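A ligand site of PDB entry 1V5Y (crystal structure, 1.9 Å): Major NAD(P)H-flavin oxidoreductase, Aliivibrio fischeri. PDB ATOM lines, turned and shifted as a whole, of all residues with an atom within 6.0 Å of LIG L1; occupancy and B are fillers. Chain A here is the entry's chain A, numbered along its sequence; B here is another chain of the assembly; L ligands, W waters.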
ATOM      1  N   LEU A   8      18.930  -3.548 -22.655  1.00  0.00           N
ATOM      2  CA  LEU A   8      18.192  -3.226 -23.866  1.00  0.00           C
ATOM      3  C   LEU A   8      17.257  -4.327 -24.347  1.00  0.00           C
ATOM      4  O   LEU A   8      16.265  -4.048 -25.016  1.00  0.00           O
ATOM      5  CB  LEU A   8      19.148  -2.770 -24.958  1.00  0.00           C
ATOM      6  CG  LEU A   8      19.883  -1.479 -24.596  1.00  0.00           C
ATOM      7  CD1 LEU A   8      20.873  -1.122 -25.675  1.00  0.00           C
ATOM      8  CD2 LEU A   8      18.899  -0.341 -24.361  1.00  0.00           C
ATOM      9  N   ARG A  11      14.160  -4.014 -21.419  1.00  0.00           N
ATOM     10  CA  ARG A  11      13.259  -2.854 -21.366  1.00  0.00           C
ATOM     11  C   ARG A  11      12.252  -3.104 -22.498  1.00  0.00           C
ATOM     12  O   ARG A  11      12.544  -3.837 -23.444  1.00  0.00           O
ATOM     13  CB  ARG A  11      14.020  -1.551 -21.620  1.00  0.00           C
ATOM     14  CG  ARG A  11      14.678  -1.463 -22.998  1.00  0.00           C
ATOM     15  CD  ARG A  11      14.705  -0.041 -23.526  1.00  0.00           C
ATOM     16  NE  ARG A  11      13.346   0.457 -23.730  1.00  0.00           N
ATOM     17  CZ  ARG A  11      12.526   0.057 -24.701  1.00  0.00           C
ATOM     18  NH1 ARG A  11      12.913  -0.859 -25.600  1.00  0.00           N
ATOM     19  NH2 ARG A  11      11.285   0.490 -24.717  1.00  0.00           N
ATOM     20  N   TYR A  12      11.043  -2.580 -22.356  1.00  0.00           N
ATOM     21  CA  TYR A  12       9.990  -2.753 -23.364  1.00  0.00           C
ATOM     22  C   TYR A  12       8.942  -1.678 -23.101  1.00  0.00           C
ATOM     23  O   TYR A  12       9.041  -0.943 -22.110  1.00  0.00           O
ATOM     24  CB  TYR A  12       9.312  -4.134 -23.240  1.00  0.00           C
ATOM     25  CG  TYR A  12       8.462  -4.274 -22.011  1.00  0.00           C
ATOM     26  CD1 TYR A  12       7.062  -4.304 -22.106  1.00  0.00           C
ATOM     27  CD2 TYR A  12       9.034  -4.280 -20.729  1.00  0.00           C
ATOM     28  CE1 TYR A  12       6.262  -4.333 -20.968  1.00  0.00           C
ATOM     29  CE2 TYR A  12       8.234  -4.309 -19.591  1.00  0.00           C
ATOM     30  CZ  TYR A  12       6.854  -4.336 -19.725  1.00  0.00           C
ATOM     31  OH  TYR A  12       6.078  -4.366 -18.606  1.00  0.00           O
ATOM     32  N   THR A  13       7.939  -1.611 -23.962  1.00  0.00           N
ATOM     33  CA  THR A  13       6.866  -0.632 -23.802  1.00  0.00           C
ATOM     34  C   THR A  13       5.738  -1.215 -22.954  1.00  0.00           C
ATOM     35  O   THR A  13       5.042  -2.161 -23.356  1.00  0.00           O
ATOM     36  CB  THR A  13       6.341  -0.122 -25.158  1.00  0.00           C
ATOM     37  OG1 THR A  13       7.395   0.581 -25.833  1.00  0.00           O
ATOM     38  CG2 THR A  13       5.120   0.809 -24.971  1.00  0.00           C
ATOM     39  N   SER A  14       5.586  -0.678 -21.758  1.00  0.00           N
ATOM     40  CA  SER A  14       4.526  -1.161 -20.864  1.00  0.00           C
ATOM     41  C   SER A  14       3.149  -0.755 -21.399  1.00  0.00           C
ATOM     42  O   SER A  14       2.968   0.358 -21.869  1.00  0.00           O
ATOM     43  CB  SER A  14       4.746  -0.580 -19.461  1.00  0.00           C
ATOM     44  OG  SER A  14       3.696  -0.973 -18.585  1.00  0.00           O
ATOM     45  N   LYS A  15       2.184  -1.677 -21.336  1.00  0.00           N
ATOM     46  CA  LYS A  15       0.824  -1.429 -21.805  1.00  0.00           C
ATOM     47  C   LYS A  15      -0.206  -1.318 -20.656  1.00  0.00           C
ATOM     48  O   LYS A  15      -1.410  -1.242 -20.920  1.00  0.00           O
ATOM     49  CB  LYS A  15       0.390  -2.523 -22.778  1.00  0.00           C
ATOM     50  CG  LYS A  15       1.284  -2.656 -24.017  1.00  0.00           C
ATOM     51  CD  LYS A  15       1.252  -1.428 -24.909  1.00  0.00           C
ATOM     52  CE  LYS A  15       2.239  -1.581 -26.053  1.00  0.00           C
ATOM     53  NZ  LYS A  15       2.155  -0.480 -27.046  1.00  0.00           N
ATOM     54  N   PHE A  71      -6.448   5.430 -26.512  1.00  0.00           N
ATOM     55  CA  PHE A  71      -5.802   4.193 -26.048  1.00  0.00           C
ATOM     56  C   PHE A  71      -4.643   4.487 -25.107  1.00  0.00           C
ATOM     57  O   PHE A  71      -4.271   3.638 -24.308  1.00  0.00           O
ATOM     58  CB  PHE A  71      -5.353   3.319 -27.228  1.00  0.00           C
ATOM     59  CG  PHE A  71      -4.165   3.858 -27.979  1.00  0.00           C
ATOM     60  CD1 PHE A  71      -2.913   3.281 -27.829  1.00  0.00           C
ATOM     61  CD2 PHE A  71      -4.297   4.954 -28.821  1.00  0.00           C
ATOM     62  CE1 PHE A  71      -1.810   3.791 -28.510  1.00  0.00           C
ATOM     63  CE2 PHE A  71      -3.194   5.464 -29.501  1.00  0.00           C
ATOM     64  CZ  PHE A  71      -1.956   4.892 -29.343  1.00  0.00           C
ATOM     65  N   ASN A  72      -4.076   5.680 -25.211  1.00  0.00           N
ATOM     66  CA  ASN A  72      -2.985   6.084 -24.330  1.00  0.00           C
ATOM     67  C   ASN A  72      -3.452   6.732 -23.011  1.00  0.00           C
ATOM     68  O   ASN A  72      -2.715   6.760 -22.030  1.00  0.00           O
ATOM     69  CB  ASN A  72      -2.060   7.074 -25.047  1.00  0.00           C
ATOM     70  CG  ASN A  72      -1.063   6.401 -25.956  1.00  0.00           C
ATOM     71  OD1 ASN A  72      -0.697   5.244 -25.758  1.00  0.00           O
ATOM     72  ND2 ASN A  72      -0.585   7.133 -26.954  1.00  0.00           N
ATOM     73  N   HIS A  75      -3.090   5.433 -18.986  1.00  0.00           N
ATOM     74  CA  HIS A  75      -1.782   5.433 -18.349  1.00  0.00           C
ATOM     75  C   HIS A  75      -1.511   6.661 -17.521  1.00  0.00           C
ATOM     76  O   HIS A  75      -0.737   6.580 -16.575  1.00  0.00           O
ATOM     77  CB  HIS A  75      -0.652   5.346 -19.392  1.00  0.00           C
ATOM     78  CG  HIS A  75      -0.755   4.167 -20.298  1.00  0.00           C
ATOM     79  ND1 HIS A  75      -1.173   2.932 -19.864  1.00  0.00           N
ATOM     80  CD2 HIS A  75      -0.553   4.056 -21.632  1.00  0.00           C
ATOM     81  CE1 HIS A  75      -1.239   2.109 -20.895  1.00  0.00           C
ATOM     82  NE2 HIS A  75      -0.871   2.764 -21.978  1.00  0.00           N
ATOM     83  N   TYR A 143      14.508  14.150 -29.376  1.00  0.00           N
ATOM     84  CA  TYR A 143      14.437  12.694 -29.542  1.00  0.00           C
ATOM     85  C   TYR A 143      15.748  12.021 -29.120  1.00  0.00           C
ATOM     86  O   TYR A 143      15.759  10.866 -28.728  1.00  0.00           O
ATOM     87  CB  TYR A 143      14.057  12.306 -30.970  1.00  0.00           C
ATOM     88  CG  TYR A 143      12.579  12.256 -31.169  1.00  0.00           C
ATOM     89  CD1 TYR A 143      11.802  13.419 -31.055  1.00  0.00           C
ATOM     90  CD2 TYR A 143      11.944  11.056 -31.460  1.00  0.00           C
ATOM     91  CE1 TYR A 143      10.425  13.384 -31.229  1.00  0.00           C
ATOM     92  CE2 TYR A 143      10.585  10.997 -31.627  1.00  0.00           C
ATOM     93  CZ  TYR A 143       9.823  12.172 -31.514  1.00  0.00           C
ATOM     94  OH  TYR A 143       8.480  12.103 -31.718  1.00  0.00           O
ATOM     95  N   LEU A 146      15.418  11.711 -25.562  1.00  0.00           N
ATOM     96  CA  LEU A 146      14.494  10.625 -25.286  1.00  0.00           C
ATOM     97  C   LEU A 146      15.202   9.267 -25.375  1.00  0.00           C
ATOM     98  O   LEU A 146      14.941   8.366 -24.548  1.00  0.00           O
ATOM     99  CB  LEU A 146      13.311  10.662 -26.248  1.00  0.00           C
ATOM    100  CG  LEU A 146      12.289   9.521 -26.236  1.00  0.00           C
ATOM    101  CD1 LEU A 146      11.597   9.359 -24.855  1.00  0.00           C
ATOM    102  CD2 LEU A 146      11.256   9.768 -27.323  1.00  0.00           C
ATOM    103  N   LEU A 150      15.428   6.600 -22.352  1.00  0.00           N
ATOM    104  CA  LEU A 150      14.985   5.217 -22.391  1.00  0.00           C
ATOM    105  C   LEU A 150      16.086   4.254 -21.925  1.00  0.00           C
ATOM    106  O   LEU A 150      15.816   3.243 -21.291  1.00  0.00           O
ATOM    107  CB  LEU A 150      14.488   4.841 -23.791  1.00  0.00           C
ATOM    108  CG  LEU A 150      13.153   5.442 -24.230  1.00  0.00           C
ATOM    109  CD1 LEU A 150      12.936   5.062 -25.687  1.00  0.00           C
ATOM    110  CD2 LEU A 150      11.978   4.947 -23.354  1.00  0.00           C
ATOM    111  N   THR A 161       6.397   4.057 -21.061  1.00  0.00           N
ATOM    112  CA  THR A 161       5.605   4.000 -22.277  1.00  0.00           C
ATOM    113  C   THR A 161       5.848   5.303 -23.017  1.00  0.00           C
ATOM    114  O   THR A 161       5.499   6.376 -22.518  1.00  0.00           O
ATOM    115  CB  THR A 161       4.095   3.881 -22.002  1.00  0.00           C
ATOM    116  OG1 THR A 161       3.846   2.814 -21.077  1.00  0.00           O
ATOM    117  CG2 THR A 161       3.311   3.608 -23.336  1.00  0.00           C
ATOM    118  N   THR A 162       6.568   5.220 -24.128  1.00  0.00           N
ATOM    119  CA  THR A 162       6.828   6.387 -24.950  1.00  0.00           C
ATOM    120  C   THR A 162       5.527   6.610 -25.706  1.00  0.00           C
ATOM    121  O   THR A 162       4.836   5.645 -26.052  1.00  0.00           O
ATOM    122  CB  THR A 162       7.957   6.165 -25.934  1.00  0.00           C
ATOM    123  OG1 THR A 162       9.099   5.673 -25.237  1.00  0.00           O
ATOM    124  CG2 THR A 162       8.327   7.470 -26.582  1.00  0.00           C
ATOM    125  N   MET A 163       5.164   7.870 -25.905  1.00  0.00           N
ATOM    126  CA  MET A 163       3.905   8.166 -26.550  1.00  0.00           C
ATOM    127  C   MET A 163       3.930   9.282 -27.587  1.00  0.00           C
ATOM    128  O   MET A 163       4.160  10.454 -27.264  1.00  0.00           O
ATOM    129  CB  MET A 163       2.830   8.507 -25.505  1.00  0.00           C
ATOM    130  CG  MET A 163       2.385   7.369 -24.602  1.00  0.00           C
ATOM    131  SD  MET A 163       1.226   7.858 -23.257  1.00  0.00           S
ATOM    132  CE  MET A 163       2.204   9.046 -22.483  1.00  0.00           C
ATOM    133  N   GLU A 164       3.717   8.896 -28.847  1.00  0.00           N
ATOM    134  CA  GLU A 164       3.602   9.860 -29.936  1.00  0.00           C
ATOM    135  C   GLU A 164       2.095  10.019 -30.214  1.00  0.00           C
ATOM    136  O   GLU A 164       1.680  10.900 -30.962  1.00  0.00           O
ATOM    137  CB  GLU A 164       4.325   9.373 -31.196  1.00  0.00           C
ATOM    138  CG  GLU A 164       5.654  10.054 -31.432  1.00  0.00           C
ATOM    139  CD  GLU A 164       6.328   9.548 -32.722  1.00  0.00           C
ATOM    140  OE1 GLU A 164       5.697   8.806 -33.511  1.00  0.00           O
ATOM    141  OE2 GLU A 164       7.498   9.915 -32.956  1.00  0.00           O
ATOM    142  N   GLY A 165       1.298   9.130 -29.641  1.00  0.00           N
ATOM    143  CA  GLY A 165      -0.148   9.164 -29.753  1.00  0.00           C
ATOM    144  C   GLY A 165      -0.703  10.160 -28.721  1.00  0.00           C
ATOM    145  O   GLY A 165      -1.341   9.763 -27.737  1.00  0.00           O
ATOM    146  N   ILE A 166      -0.380  11.432 -28.915  1.00  0.00           N
ATOM    147  CA  ILE A 166      -0.811  12.532 -28.059  1.00  0.00           C
ATOM    148  C   ILE A 166      -1.374  13.647 -28.952  1.00  0.00           C
ATOM    149  O   ILE A 166      -1.236  13.585 -30.169  1.00  0.00           O
ATOM    150  CB  ILE A 166       0.358  13.138 -27.194  1.00  0.00           C
ATOM    151  CG1 ILE A 166       1.459  13.703 -28.082  1.00  0.00           C
ATOM    152  CG2 ILE A 166       0.924  12.095 -26.234  1.00  0.00           C
ATOM    153  CD1 ILE A 166       2.563  14.409 -27.327  1.00  0.00           C
ATOM    154  N   VAL A 186       6.084  14.278 -28.276  1.00  0.00           N
ATOM    155  CA  VAL A 186       6.268  13.002 -27.627  1.00  0.00           C
ATOM    156  C   VAL A 186       6.298  13.165 -26.110  1.00  0.00           C
ATOM    157  O   VAL A 186       6.790  14.153 -25.581  1.00  0.00           O
ATOM    158  CB  VAL A 186       7.547  12.289 -28.175  1.00  0.00           C
ATOM    159  CG1 VAL A 186       8.791  13.057 -27.831  1.00  0.00           C
ATOM    160  CG2 VAL A 186       7.611  10.853 -27.707  1.00  0.00           C
ATOM    161  N   ASN A 200       2.245  -6.900 -22.675  1.00  0.00           N
ATOM    162  CA  ASN A 200       3.480  -6.758 -23.389  1.00  0.00           C
ATOM    163  C   ASN A 200       4.689  -7.234 -22.628  1.00  0.00           C
ATOM    164  O   ASN A 200       5.744  -7.436 -23.212  1.00  0.00           O
ATOM    165  CB  ASN A 200       3.687  -5.323 -23.832  1.00  0.00           C
ATOM    166  CG  ASN A 200       4.444  -5.230 -25.131  1.00  0.00           C
ATOM    167  OD1 ASN A 200       4.351  -6.118 -25.965  1.00  0.00           O
ATOM    168  ND2 ASN A 200       5.207  -4.170 -25.313  1.00  0.00           N
ATOM    169  N   LYS A 205      10.558  -9.627 -27.754  1.00  0.00           N
ATOM    170  CA  LYS A 205      10.904  -8.376 -28.403  1.00  0.00           C
ATOM    171  C   LYS A 205      11.186  -8.755 -29.867  1.00  0.00           C
ATOM    172  O   LYS A 205      11.674  -9.865 -30.131  1.00  0.00           O
ATOM    173  CB  LYS A 205      12.137  -7.725 -27.768  1.00  0.00           C
ATOM    174  CG  LYS A 205      12.526  -6.377 -28.403  1.00  0.00           C
ATOM    175  CD  LYS A 205      13.594  -5.616 -27.632  1.00  0.00           C
ATOM    176  CE  LYS A 205      13.197  -5.370 -26.169  1.00  0.00           C
ATOM    177  NZ  LYS A 205      11.853  -4.739 -26.021  1.00  0.00           N
ATOM    178  N   SER A 206      10.821  -7.875 -30.796  1.00  0.00           N
ATOM    179  CA  SER A 206      11.046  -8.133 -32.220  1.00  0.00           C
ATOM    180  C   SER A 206      11.691  -6.948 -32.920  1.00  0.00           C
ATOM    181  O   SER A 206      11.250  -5.809 -32.761  1.00  0.00           O
ATOM    182  CB  SER A 206       9.734  -8.518 -32.918  1.00  0.00           C
ATOM    183  OG  SER A 206       9.980  -8.905 -34.271  1.00  0.00           O
ATOM    184  N   ARG A 207      12.804  -7.225 -33.606  1.00  0.00           N
ATOM    185  CA  ARG A 207      13.535  -6.223 -34.373  1.00  0.00           C
ATOM    186  C   ARG A 207      13.938  -6.868 -35.699  1.00  0.00           C
ATOM    187  O   ARG A 207      13.957  -8.100 -35.833  1.00  0.00           O
ATOM    188  CB  ARG A 207      14.797  -5.762 -33.634  1.00  0.00           C
ATOM    189  CG  ARG A 207      14.552  -4.926 -32.346  1.00  0.00           C
ATOM    190  CD  ARG A 207      13.796  -3.618 -32.630  1.00  0.00           C
ATOM    191  NE  ARG A 207      13.747  -2.792 -31.426  1.00  0.00           N
ATOM    192  CZ  ARG A 207      12.837  -2.889 -30.478  1.00  0.00           C
ATOM    193  NH1 ARG A 207      11.857  -3.770 -30.590  1.00  0.00           N
ATOM    194  NH2 ARG A 207      12.942  -2.134 -29.379  1.00  0.00           N
ATOM    195  N   LEU B  37      18.535  -2.783 -31.218  1.00  0.00           N
ATOM    196  CA  LEU B  37      17.498  -2.902 -30.205  1.00  0.00           C
ATOM    197  C   LEU B  37      16.780  -1.592 -29.850  1.00  0.00           C
ATOM    198  O   LEU B  37      15.878  -1.607 -29.032  1.00  0.00           O
ATOM    199  CB  LEU B  37      18.075  -3.513 -28.936  1.00  0.00           C
ATOM    200  CG  LEU B  37      18.546  -4.959 -29.098  1.00  0.00           C
ATOM    201  CD1 LEU B  37      19.338  -5.372 -27.853  1.00  0.00           C
ATOM    202  CD2 LEU B  37      17.354  -5.860 -29.327  1.00  0.00           C
ATOM    203  N   SER B  38      17.179  -0.485 -30.473  1.00  0.00           N
ATOM    204  CA  SER B  38      16.561   0.829 -30.223  1.00  0.00           C
ATOM    205  C   SER B  38      15.068   0.812 -30.493  1.00  0.00           C
ATOM    206  O   SER B  38      14.588   0.172 -31.434  1.00  0.00           O
ATOM    207  CB  SER B  38      17.180   1.913 -31.089  1.00  0.00           C
ATOM    208  OG  SER B  38      18.565   2.029 -30.871  1.00  0.00           O
ATOM    209  N   ALA B  39      14.331   1.527 -29.643  1.00  0.00           N
ATOM    210  CA  ALA B  39      12.890   1.622 -29.777  1.00  0.00           C
ATOM    211  C   ALA B  39      12.561   2.647 -30.867  1.00  0.00           C
ATOM    212  O   ALA B  39      13.367   3.530 -31.161  1.00  0.00           O
ATOM    213  CB  ALA B  39      12.278   2.062 -28.426  1.00  0.00           C
ATOM    214  N   SER B  40      11.395   2.514 -31.484  1.00  0.00           N
ATOM    215  CA  SER B  40      10.982   3.473 -32.505  1.00  0.00           C
ATOM    216  C   SER B  40       9.487   3.424 -32.563  1.00  0.00           C
ATOM    217  O   SER B  40       8.880   2.422 -32.165  1.00  0.00           O
ATOM    218  CB  SER B  40      11.594   3.154 -33.872  1.00  0.00           C
ATOM    219  OG  SER B  40      11.235   1.861 -34.303  1.00  0.00           O
ATOM    220  N   SER B  41       8.883   4.515 -33.023  1.00  0.00           N
ATOM    221  CA  SER B  41       7.435   4.604 -33.158  1.00  0.00           C
ATOM    222  C   SER B  41       6.952   3.434 -34.006  1.00  0.00           C
ATOM    223  O   SER B  41       7.471   3.204 -35.082  1.00  0.00           O
ATOM    224  CB  SER B  41       7.059   5.925 -33.833  1.00  0.00           C
ATOM    225  OG  SER B  41       5.652   6.088 -33.846  1.00  0.00           O
ATOM    226  N   ILE B  42       5.923   2.747 -33.517  1.00  0.00           N
ATOM    227  CA  ILE B  42       5.329   1.531 -34.109  1.00  0.00           C
ATOM    228  C   ILE B  42       6.334   0.434 -34.525  1.00  0.00           C
ATOM    229  O   ILE B  42       5.992  -0.442 -35.311  1.00  0.00           O
ATOM    230  CB  ILE B  42       4.266   1.816 -35.257  1.00  0.00           C
ATOM    231  CG1 ILE B  42       4.929   2.307 -36.557  1.00  0.00           C
ATOM    232  CG2 ILE B  42       3.217   2.825 -34.774  1.00  0.00           C
ATOM    233  CD1 ILE B  42       4.050   2.199 -37.780  1.00  0.00           C
ATOM    234  N   ASN B  43       7.516   0.439 -33.911  1.00  0.00           N
ATOM    235  CA  ASN B  43       8.580  -0.521 -34.208  1.00  0.00           C
ATOM    236  C   ASN B  43       8.945  -0.442 -35.682  1.00  0.00           C
ATOM    237  O   ASN B  43       9.439  -1.399 -36.275  1.00  0.00           O
ATOM    238  CB  ASN B  43       8.155  -1.948 -33.857  1.00  0.00           C
ATOM    239  CG  ASN B  43       9.348  -2.872 -33.627  1.00  0.00           C
ATOM    240  OD1 ASN B  43      10.431  -2.401 -33.306  1.00  0.00           O
ATOM    241  ND2 ASN B  43       9.145  -4.174 -33.807  1.00  0.00           N
ATOM    242  N   ARG B 108       5.116 -12.543 -31.563  1.00  0.00           N
ATOM    243  CA  ARG B 108       4.461 -11.527 -30.750  1.00  0.00           C
ATOM    244  C   ARG B 108       3.033 -11.252 -31.220  1.00  0.00           C
ATOM    245  O   ARG B 108       2.179 -10.848 -30.426  1.00  0.00           O
ATOM    246  CB  ARG B 108       5.306 -10.281 -30.471  1.00  0.00           C
ATOM    247  CG  ARG B 108       5.966  -9.594 -31.598  1.00  0.00           C
ATOM    248  CD  ARG B 108       6.690  -8.359 -31.050  1.00  0.00           C
ATOM    249  NE  ARG B 108       5.762  -7.362 -30.513  1.00  0.00           N
ATOM    250  CZ  ARG B 108       5.673  -6.997 -29.234  1.00  0.00           C
ATOM    251  NH1 ARG B 108       6.476  -7.544 -28.318  1.00  0.00           N
ATOM    252  NH2 ARG B 108       4.742  -6.133 -28.853  1.00  0.00           N
ATOM    253  N   GLN B 141      13.391   9.409 -35.231  1.00  0.00           N
ATOM    254  CA  GLN B 141      13.571   8.018 -34.763  1.00  0.00           C
ATOM    255  C   GLN B 141      15.054   7.674 -34.776  1.00  0.00           C
ATOM    256  O   GLN B 141      15.561   7.045 -33.849  1.00  0.00           O
ATOM    257  CB  GLN B 141      12.828   7.010 -35.628  1.00  0.00           C
ATOM    258  CG  GLN B 141      11.381   7.340 -35.988  1.00  0.00           C
ATOM    259  CD  GLN B 141      10.484   7.563 -34.779  1.00  0.00           C
ATOM    260  OE1 GLN B 141      10.519   6.809 -33.814  1.00  0.00           O
ATOM    261  NE2 GLN B 141       9.650   8.596 -34.858  1.00  0.00           N
ATOM    262  N   LEU B 144      16.850   9.154 -31.910  1.00  0.00           N
ATOM    263  CA  LEU B 144      16.577   8.428 -30.690  1.00  0.00           C
ATOM    264  C   LEU B 144      17.634   7.319 -30.597  1.00  0.00           C
ATOM    265  O   LEU B 144      18.171   7.064 -29.531  1.00  0.00           O
ATOM    266  CB  LEU B 144      15.181   7.835 -30.736  1.00  0.00           C
ATOM    267  CG  LEU B 144      14.653   7.184 -29.451  1.00  0.00           C
ATOM    268  CD1 LEU B 144      13.156   7.027 -29.578  1.00  0.00           C
ATOM    269  CD2 LEU B 144      15.318   5.816 -29.152  1.00  0.00           C
HETATM  270  N1  LIG L   1       3.566   2.857 -27.628  1.00  0.00           N
HETATM  271  C1  LIG L   1       2.337   3.131 -27.064  1.00  0.00           C
HETATM  272  O1  LIG L   1       1.646   2.239 -26.595  1.00  0.00           O
HETATM  273  N2  LIG L   1       1.779   4.311 -27.550  1.00  0.00           N
HETATM  274  C2  LIG L   1       2.442   5.295 -28.248  1.00  0.00           C
HETATM  275  O2  LIG L   1       1.779   6.313 -28.503  1.00  0.00           O
HETATM  276  C3  LIG L   1       3.784   4.942 -28.661  1.00  0.00           C
HETATM  277  N3  LIG L   1       4.503   5.920 -29.301  1.00  0.00           N
HETATM  278  C4  LIG L   1       5.822   5.773 -29.545  1.00  0.00           C
HETATM  279  C5  LIG L   1       6.560   6.834 -29.934  1.00  0.00           C
HETATM  280  C6  LIG L   1       7.921   6.691 -30.042  1.00  0.00           C
HETATM  281  C7  LIG L   1       8.804   7.830 -30.569  1.00  0.00           C
HETATM  282  C8  LIG L   1       8.534   5.471 -29.707  1.00  0.00           C
HETATM  283  C9  LIG L   1      10.070   5.306 -29.621  1.00  0.00           C
HETATM  284  C10 LIG L   1       7.786   4.429 -29.272  1.00  0.00           C
HETATM  285  C11 LIG L   1       6.441   4.565 -29.181  1.00  0.00           C
HETATM  286  N4  LIG L   1       5.692   3.549 -28.649  1.00  0.00           N
HETATM  287  C12 LIG L   1       4.398   3.740 -28.309  1.00  0.00           C
HETATM  288  C13 LIG L   1       6.231   2.309 -28.378  1.00  0.00           C
HETATM  289  C14 LIG L   1       6.752   1.483 -29.613  1.00  0.00           C
HETATM  290  O3  LIG L   1       5.651   0.820 -30.223  1.00  0.00           O
HETATM  291  C15 LIG L   1       7.870   0.497 -29.141  1.00  0.00           C
HETATM  292  O4  LIG L   1       8.959   1.254 -28.664  1.00  0.00           O
HETATM  293  C16 LIG L   1       8.388  -0.408 -30.339  1.00  0.00           C
HETATM  294  O5  LIG L   1       7.263  -1.261 -30.705  1.00  0.00           O
HETATM  295  C17 LIG L   1       9.520  -1.308 -29.863  1.00  0.00           C
HETATM  296  O6  LIG L   1       9.102  -2.077 -28.698  1.00  0.00           O
HETATM  297  P1  LIG L   1       9.704  -2.000 -27.194  1.00  0.00           P
HETATM  298  O7  LIG L   1       8.698  -2.882 -26.559  1.00  0.00           O
HETATM  299  O8  LIG L   1       9.625  -0.519 -27.005  1.00  0.00           O
HETATM  300  O9  LIG L   1      11.083  -2.485 -27.494  1.00  0.00           O
HETATM  301  C1  LG2 L   2       2.165   2.068 -30.742  1.00  0.00           C
HETATM  302  C2  LG2 L   2       0.794   2.216 -30.728  1.00  0.00           C
HETATM  303  C3  LG2 L   2       1.008   4.464 -31.571  1.00  0.00           C
HETATM  304  C4  LG2 L   2       2.367   4.272 -31.669  1.00  0.00           C
HETATM  305  C5  LG2 L   2       2.946   3.072 -31.269  1.00  0.00           C
HETATM  306  C6  LG2 L   2       0.416   5.689 -31.895  1.00  0.00           C
HETATM  307  C7  LG2 L   2       1.176   6.623 -32.573  1.00  0.00           C
HETATM  308  C8  LG2 L   2       2.557   6.495 -32.590  1.00  0.00           C
HETATM  309  C9  LG2 L   2       3.158   5.299 -32.179  1.00  0.00           C
HETATM  310  O1  LG2 L   2       0.095   1.289 -30.364  1.00  0.00           O
HETATM  311  O2  LG2 L   2       0.216   3.415 -31.138  1.00  0.00           O
HETATM  312  O3  LG2 L   2       4.275   2.851 -31.394  1.00  0.00           O
HETATM  313  O   HOH W   1       6.213  -3.290 -27.734  1.00  0.00           O
HETATM  314  O   HOH W   2       4.520  -1.076 -28.427  1.00  0.00           O
HETATM  315  O   HOH W   3       9.319  -5.502 -26.847  1.00  0.00           O
HETATM  316  O   HOH W   4      -0.542   2.534 -24.939  1.00  0.00           O
HETATM  317  O   HOH W   5       7.004  -4.155 -30.764  1.00  0.00           O
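ND2 of Asn 72 lies within hydrogen-bond range of O2 of LIG L1.
An oxygen (O2) of LIG L1 sits at hydrogen-bond distance from the backbone NH (N) of Gly 165 (3.1 Å).
N of Glu 164 sits at hydrogen-bond distance from N3 of LIG L1, 3.1 Å away.
The side-chain amino group (NZ) of Lys 15 lies within hydrogen-bond range of an oxygen (O1) of LIG L1 (2.8 Å).
NZ of Lys 205 is in salt-bridge range of O9 of LIG L1 (2.8 Å).
O8 of LIG L1 lies within hydrogen-bond range of OG1 of Thr 13 (2.7 Å).
The guanidinium group (NH2) of Arg 11 is in salt-bridge range of an oxygen (O8) of LIG L1 (3.0 Å).
The backbone NH (N) of Thr 13 is in hydrogen-bond range of an oxygen (O7) of LIG L1, at 3.0 Å.
The backbone NH of Ile 42 of chain B sits at hydrogen-bond distance from an oxygen (O3) of LG2 L2, at 2.7 Å.
The guanidinium group of Arg 207 lies within salt-bridge range of an oxygen (O9) of LIG L1.
An oxygen (O3) of LIG L1 lies within hydrogen-bond range of an oxygen (O3) of LG2 L2, at 2.7 Å.
The side-chain carboxylate (OE1) of Glu 164 lies within hydrogen-bond range of the side-chain hydroxyl (OG) of Ser 41 of chain B, at 2.7 Å.
The backbone carbonyl oxygen (O) of Thr 13 lies within hydrogen-bond range of the side-chain amide nitrogen (ND2) of Asn 200 (2.8 Å).
ND2 of Asn 43 of chain B lies within hydrogen-bond range of O of Ser 206, at 2.9 Å.
The side-chain amide oxygen of Asn 43 of chain B sits at hydrogen-bond distance from the guanidinium group of Arg 207, 3.4 Å away.
OE2 of Glu 164 lies within hydrogen-bond range of NE2 of Gln 141 of chain B, 3.2 Å away.
NE of Arg 207 is in hydrogen-bond range of O of Ser 38 of chain B (3.1 Å).
The backbone carbonyl oxygen of Ser 14 is in hydrogen-bond range of the side-chain hydroxyl of Thr 161 (2.7 Å).
The side-chain amide nitrogen (ND2) of Asn 72 lies within hydrogen-bond range of the backbone carbonyl oxygen (O) of Gly 165.
A nitrogen (N3) of LIG L1 sits close to the backbone carbonyl oxygen (O) of Thr 162.
Merely in contact with LIG L1: Asn 43 of chain B (3.3 Å), Ser 40 of chain B (3.4 Å), Ala 39 of chain B (3.4 Å), Met 163 (3.4 Å), Tyr 12 (3.4 Å), Ser 41 of chain B (3.5 Å), Leu 144 of chain B (3.5 Å), Phe 71 (3.8 Å), Tyr 143 (3.8 Å), Gln 141 of chain B (3.8 Å), Ile 42 of chain B (3.8 Å), Thr 161 (3.9 Å) and Asn 200 (3.9 Å).
Of the 33 residues printed, 22 come within 4 Å of LIG L1.
Water W3 lies within hydrogen-bond range of an oxygen (O7) of LIG L1 (2.7 Å) and the side-chain amino group of Lys 205 (2.8 Å).
Water W4 lies within hydrogen-bond range of O1 of LIG L1, OD1 of Asn 72 and NE2 of His 75.
Water W1 lies within hydrogen-bond range of the side-chain amide nitrogen of Asn 200 (2.8 Å), an oxygen (O7) of LIG L1 (2.8 Å) and the guanidinium group of Arg 108 of chain B (3.4 Å).
Water W2 bridges NZ of Lys 15 (2.8 Å) and O3 of LIG L1 (2.8 Å).
Water W5 bridges an oxygen (O5) of LIG L1 (2.9 Å) and the guanidinium group (NE) of Arg 108 of chain B (3.4 Å).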
